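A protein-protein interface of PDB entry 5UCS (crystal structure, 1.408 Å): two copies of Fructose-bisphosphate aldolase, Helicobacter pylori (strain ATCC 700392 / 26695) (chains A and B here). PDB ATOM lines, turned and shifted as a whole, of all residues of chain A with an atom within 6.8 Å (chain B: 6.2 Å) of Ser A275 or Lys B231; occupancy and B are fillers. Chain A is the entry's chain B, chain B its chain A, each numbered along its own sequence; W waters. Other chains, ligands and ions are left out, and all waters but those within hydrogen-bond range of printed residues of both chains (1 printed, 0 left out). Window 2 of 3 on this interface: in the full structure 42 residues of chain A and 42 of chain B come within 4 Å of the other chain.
Gly B228 touches Lys A274 (CA to O, 3.3 Å). OH of Tyr B223 touches C of Ser A275, at 3.6 Å. Ser A275 touches Asp B229 (CA to O, 3.1 Å). CD2 of Phe A277 touches OH of Tyr B223 (3.8 Å). CE2 of Phe A277 touches CD2 of Leu B230 (3.9 Å).
Water W1 bridges NH1 of Arg B267 (2.9 Å) and NZ of Lys A274 (3.3 Å).
O of Tyr B223 is in hydrogen-bond range of N of Gly B228, 3.0 Å away. NE of Arg B267 lies within hydrogen-bond range of OH of Tyr B223. OD2 of Asp B229 lies within hydrogen-bond range of N of Lys B231 (2.8 Å). The side-chain hydroxyl of Ser B233 lies within hydrogen-bond range of the backbone carbonyl oxygen of Leu B230 (2.7 Å). The side-chain carboxylate (OD1) of Asp A273 is in hydrogen-bond range of the side-chain hydroxyl (OG) of Ser A275 (2.6 Å). OE1 of Gln A276 lies within hydrogen-bond range of N of Asp A278.
The side-chain hydroxyl (OH) of Tyr B223 sits at hydrogen-bond distance from the backbone carbonyl oxygen (O) of Lys A274 (2.9 Å). O of Gln A276 sits at hydrogen-bond distance from OH of Tyr B223. O of Lys A274 lies within hydrogen-bond range of N of Asp B229 (2.9 Å). OG of Ser A275 lies close to NZ of Lys B231. The backbone carbonyl oxygen (O) of Ala A270 is in hydrogen-bond range of the guanidinium group (NH1) of Arg B267, 2.8 Å away. The guanidinium group (NH2) of Arg B267 sits at hydrogen-bond distance from the backbone carbonyl oxygen (O) of Asp A273 (2.8 Å). The guanidinium group of Arg B267 is in hydrogen-bond range of the backbone carbonyl oxygen of Lys A274 (3.5 Å). The guanidinium group (NH2) of Arg B267 sits at hydrogen-bond distance from the backbone carbonyl oxygen (O) of Gln A276 (2.9 Å).
No position is printed for both chains. Of the 13 pairs that touch across the chains among the printed residues, none has its exchanged pair printed and touching as well.
Ser A275 touches three residues of chain B. Of the printed residues of chain A, Lys B231 touches Ser A275 (3.2 Å). Of the printed residues of chain B, Lys A274 touches Tyr B223 (2.9 Å), Gly B228 (3.3 Å), Asp B229 (2.9 Å) and Arg B267 (3.5 Å). Of the printed residues of chain B, Phe A277 touches Tyr B223 (3.8 Å) and Leu B230 (3.9 Å). Of the printed residues of chain B, Gln A276 touches Tyr B223 (3.1 Å) and Arg B267 (2.9 Å). Of the printed residues of chain B, Asp A273 touches Arg B267. Asp A278 touches none of the printed residues of chain B. Gly B232 touches none of the printed residues of chain A. The nearest printed residue of chain A that does not touch Tyr B223 is Asp A273 (5.2 Å).
Of the 8 printed residues of chain A, 6 touch a printed residue of chain B. Printed residues of chain A that touch a printed residue of chain B: Ala A270, Asp A273, Lys A274, Ser A275, Gln A276 and Phe A277. Among the printed residues, no Asp or Glu carboxylate lies within 4 Å of a Lys or Arg side-chain nitrogen of the other chain.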
ATOM      1  N   ALA A 270       6.144  22.560  34.859  1.00  0.00           N
ATOM      2  CA  ALA A 270       5.418  23.417  33.936  1.00  0.00           C
ATOM      3  C   ALA A 270       6.338  24.450  33.307  1.00  0.00           C
ATOM      4  O   ALA A 270       6.241  24.724  32.100  1.00  0.00           O
ATOM      5  CB  ALA A 270       4.280  24.107  34.671  1.00  0.00           C
ATOM      6  N   GLU A 272       9.696  24.330  32.875  1.00  0.00           N
ATOM      7  CA  GLU A 272      10.877  23.849  32.161  1.00  0.00           C
ATOM      8  C   GLU A 272      10.563  23.103  30.874  1.00  0.00           C
ATOM      9  O   GLU A 272      11.471  22.919  30.054  1.00  0.00           O
ATOM     10  CB  GLU A 272      11.736  22.968  33.072  1.00  0.00           C
ATOM     11  CG  GLU A 272      12.371  23.776  34.221  1.00  0.00           C
ATOM     12  CD  GLU A 272      13.286  22.968  35.122  1.00  0.00           C
ATOM     13  OE1 GLU A 272      13.191  21.730  35.130  1.00  0.00           O
ATOM     14  OE2 GLU A 272      14.098  23.590  35.838  1.00  0.00           O
ATOM     15  N   ASP A 273       9.320  22.666  30.670  1.00  0.00           N
ATOM     16  CA  ASP A 273       8.934  22.015  29.415  1.00  0.00           C
ATOM     17  C   ASP A 273       7.481  22.396  29.155  1.00  0.00           C
ATOM     18  O   ASP A 273       6.569  21.809  29.739  1.00  0.00           O
ATOM     19  CB  ASP A 273       9.099  20.503  29.472  1.00  0.00           C
ATOM     20  CG  ASP A 273       8.819  19.837  28.138  1.00  0.00           C
ATOM     21  OD1 ASP A 273       8.371  20.534  27.200  1.00  0.00           O
ATOM     22  OD2 ASP A 273       9.077  18.622  28.012  1.00  0.00           O
ATOM     23  N   LYS A 274       7.279  23.369  28.273  1.00  0.00           N
ATOM     24  CA  LYS A 274       5.930  23.792  27.931  1.00  0.00           C
ATOM     25  C   LYS A 274       5.140  22.727  27.172  1.00  0.00           C
ATOM     26  O   LYS A 274       3.914  22.840  27.101  1.00  0.00           O
ATOM     27  CB  LYS A 274       5.992  25.088  27.124  1.00  0.00           C
ATOM     28  CG  LYS A 274       6.688  26.234  27.841  1.00  0.00           C
ATOM     29  CD  LYS A 274       5.991  26.574  29.144  1.00  0.00           C
ATOM     30  CE  LYS A 274       6.541  27.845  29.758  1.00  0.00           C
ATOM     31  NZ  LYS A 274       5.701  28.295  30.905  1.00  0.00           N
ATOM     32  N   SER A 275       5.791  21.687  26.659  1.00  0.00           N
ATOM     33  CA  SER A 275       5.105  20.603  25.965  1.00  0.00           C
ATOM     34  C   SER A 275       4.714  19.456  26.884  1.00  0.00           C
ATOM     35  O   SER A 275       4.089  18.496  26.424  1.00  0.00           O
ATOM     36  CB  SER A 275       5.967  20.056  24.817  1.00  0.00           C
ATOM     37  OG  SER A 275       7.061  19.279  25.307  1.00  0.00           O
ATOM     38  N   GLN A 276       5.042  19.530  28.173  1.00  0.00           N
ATOM     39  CA  GLN A 276       4.831  18.406  29.081  1.00  0.00           C
ATOM     40  C   GLN A 276       3.391  18.370  29.568  1.00  0.00           C
ATOM     41  O   GLN A 276       2.917  19.321  30.199  1.00  0.00           O
ATOM     42  CB  GLN A 276       5.778  18.498  30.279  1.00  0.00           C
ATOM     43  CG  GLN A 276       5.701  17.275  31.205  1.00  0.00           C
ATOM     44  CD  GLN A 276       6.018  15.978  30.469  1.00  0.00           C
ATOM     45  OE1 GLN A 276       5.134  15.257  30.004  1.00  0.00           O
ATOM     46  NE2 GLN A 276       7.310  15.680  30.366  1.00  0.00           N
ATOM     47  N   PHE A 277       2.693  17.262  29.282  1.00  0.00           N
ATOM     48  CA  PHE A 277       1.365  17.042  29.846  1.00  0.00           C
ATOM     49  C   PHE A 277       1.141  15.611  30.332  1.00  0.00           C
ATOM     50  O   PHE A 277      -0.004  15.226  30.582  1.00  0.00           O
ATOM     51  CB  PHE A 277       0.260  17.490  28.896  1.00  0.00           C
ATOM     52  CG  PHE A 277       0.397  16.951  27.494  1.00  0.00           C
ATOM     53  CD1 PHE A 277      -0.001  15.660  27.182  1.00  0.00           C
ATOM     54  CD2 PHE A 277       0.910  17.747  26.497  1.00  0.00           C
ATOM     55  CE1 PHE A 277       0.115  15.171  25.885  1.00  0.00           C
ATOM     56  CE2 PHE A 277       1.032  17.277  25.197  1.00  0.00           C
ATOM     57  CZ  PHE A 277       0.633  15.990  24.895  1.00  0.00           C
ATOM     58  N   ASP A 278       2.207  14.839  30.541  1.00  0.00           N
ATOM     59  CA  ASP A 278       2.105  13.562  31.226  1.00  0.00           C
ATOM     60  C   ASP A 278       1.986  13.855  32.720  1.00  0.00           C
ATOM     61  O   ASP A 278       2.915  14.407  33.319  1.00  0.00           O
ATOM     62  CB  ASP A 278       3.354  12.741  30.893  1.00  0.00           C
ATOM     63  CG  ASP A 278       3.387  11.371  31.558  1.00  0.00           C
ATOM     64  OD1 ASP A 278       2.609  11.080  32.485  1.00  0.00           O
ATOM     65  OD2 ASP A 278       4.240  10.564  31.120  1.00  0.00           O
ATOM     66  N   TYR B 223      -4.790  25.042  26.391  1.00  0.00           N
ATOM     67  CA  TYR B 223      -3.404  24.675  26.651  1.00  0.00           C
ATOM     68  C   TYR B 223      -2.436  25.772  26.209  1.00  0.00           C
ATOM     69  O   TYR B 223      -1.523  26.147  26.960  1.00  0.00           O
ATOM     70  CB  TYR B 223      -3.098  23.341  25.977  1.00  0.00           C
ATOM     71  CG  TYR B 223      -1.808  22.747  26.460  1.00  0.00           C
ATOM     72  CD1 TYR B 223      -1.761  22.089  27.682  1.00  0.00           C
ATOM     73  CD2 TYR B 223      -0.631  22.860  25.736  1.00  0.00           C
ATOM     74  CE1 TYR B 223      -0.587  21.554  28.169  1.00  0.00           C
ATOM     75  CE2 TYR B 223       0.554  22.317  26.211  1.00  0.00           C
ATOM     76  CZ  TYR B 223       0.573  21.675  27.442  1.00  0.00           C
ATOM     77  OH  TYR B 223       1.740  21.143  27.945  1.00  0.00           O
ATOM     78  N   GLY B 228       1.381  26.685  27.110  1.00  0.00           N
ATOM     79  CA  GLY B 228       1.833  25.406  26.615  1.00  0.00           C
ATOM     80  C   GLY B 228       2.332  25.467  25.181  1.00  0.00           C
ATOM     81  O   GLY B 228       2.159  26.444  24.455  1.00  0.00           O
ATOM     82  N   ASP B 229       2.967  24.367  24.780  1.00  0.00           N
ATOM     83  CA  ASP B 229       3.501  24.171  23.435  1.00  0.00           C
ATOM     84  C   ASP B 229       3.049  22.785  23.003  1.00  0.00           C
ATOM     85  O   ASP B 229       3.317  21.803  23.701  1.00  0.00           O
ATOM     86  CB  ASP B 229       5.037  24.240  23.509  1.00  0.00           C
ATOM     87  CG  ASP B 229       5.735  23.900  22.192  1.00  0.00           C
ATOM     88  OD1 ASP B 229       6.989  23.888  22.186  1.00  0.00           O
ATOM     89  OD2 ASP B 229       5.063  23.658  21.171  1.00  0.00           O
ATOM     90  N   LEU B 230       2.325  22.696  21.886  1.00  0.00           N
ATOM     91  CA  LEU B 230       1.869  21.396  21.407  1.00  0.00           C
ATOM     92  C   LEU B 230       2.739  20.845  20.281  1.00  0.00           C
ATOM     93  O   LEU B 230       2.233  20.145  19.399  1.00  0.00           O
ATOM     94  CB  LEU B 230       0.385  21.429  21.043  1.00  0.00           C
ATOM     95  CG  LEU B 230      -0.515  21.464  22.288  1.00  0.00           C
ATOM     96  CD1 LEU B 230      -1.952  21.831  21.932  1.00  0.00           C
ATOM     97  CD2 LEU B 230      -0.480  20.119  23.008  1.00  0.00           C
ATOM     98  N   LYS B 231       4.043  21.146  20.321  1.00  0.00           N
ATOM     99  CA  LYS B 231       5.085  20.530  19.498  1.00  0.00           C
ATOM    100  C   LYS B 231       4.561  19.904  18.214  1.00  0.00           C
ATOM    101  O   LYS B 231       4.678  18.690  18.016  1.00  0.00           O
ATOM    102  CB  LYS B 231       5.849  19.475  20.311  1.00  0.00           C
ATOM    103  CG  LYS B 231       6.913  20.045  21.244  1.00  0.00           C
ATOM    104  CD  LYS B 231       7.683  18.946  21.959  1.00  0.00           C
ATOM    105  CE  LYS B 231       8.895  19.503  22.695  1.00  0.00           C
ATOM    106  NZ  LYS B 231       9.639  18.441  23.430  1.00  0.00           N
ATOM    107  N   GLY B 232       3.975  20.721  17.345  1.00  0.00           N
ATOM    108  CA  GLY B 232       3.506  20.254  16.054  1.00  0.00           C
ATOM    109  C   GLY B 232       2.692  18.974  16.083  1.00  0.00           C
ATOM    110  O   GLY B 232       2.657  18.244  15.088  1.00  0.00           O
ATOM    111  N   SER B 233       2.037  18.683  17.206  1.00  0.00           N
ATOM    112  CA  SER B 233       1.155  17.528  17.303  1.00  0.00           C
ATOM    113  C   SER B 233      -0.250  17.944  16.897  1.00  0.00           C
ATOM    114  O   SER B 233      -0.799  18.912  17.433  1.00  0.00           O
ATOM    115  CB  SER B 233       1.139  16.961  18.721  1.00  0.00           C
ATOM    116  OG  SER B 233       0.697  17.930  19.653  1.00  0.00           O
ATOM    117  N   LYS B 234      -0.820  17.219  15.943  1.00  0.00           N
ATOM    118  CA  LYS B 234      -2.152  17.502  15.439  1.00  0.00           C
ATOM    119  C   LYS B 234      -3.051  16.319  15.754  1.00  0.00           C
ATOM    120  O   LYS B 234      -2.607  15.166  15.740  1.00  0.00           O
ATOM    121  CB  LYS B 234      -2.123  17.740  13.925  1.00  0.00           C
ATOM    122  CG  LYS B 234      -2.955  18.927  13.455  1.00  0.00           C
ATOM    123  CD  LYS B 234      -2.076  20.025  12.867  1.00  0.00           C
ATOM    124  CE  LYS B 234      -1.473  19.609  11.529  1.00  0.00           C
ATOM    125  NZ  LYS B 234      -0.479  20.598  11.025  1.00  0.00           N
ATOM    126  N   ARG B 267      -1.597  24.550  34.530  1.00  0.00           N
ATOM    127  CA  ARG B 267      -0.722  25.626  34.083  1.00  0.00           C
ATOM    128  C   ARG B 267      -1.366  26.984  34.312  1.00  0.00           C
ATOM    129  O   ARG B 267      -0.705  27.917  34.781  1.00  0.00           O
ATOM    130  CB  ARG B 267      -0.369  25.445  32.602  1.00  0.00           C
ATOM    131  CG  ARG B 267       0.576  24.279  32.292  1.00  0.00           C
ATOM    132  CD  ARG B 267       0.872  24.140  30.791  1.00  0.00           C
ATOM    133  NE  ARG B 267       1.793  23.030  30.552  1.00  0.00           N
ATOM    134  CZ  ARG B 267       3.118  23.117  30.678  1.00  0.00           C
ATOM    135  NH1 ARG B 267       3.701  24.273  31.002  1.00  0.00           N
ATOM    136  NH2 ARG B 267       3.842  22.040  30.494  1.00  0.00           N
HETATM  137  O   HOH W   1       2.690  26.949  31.111  1.00  0.00           O
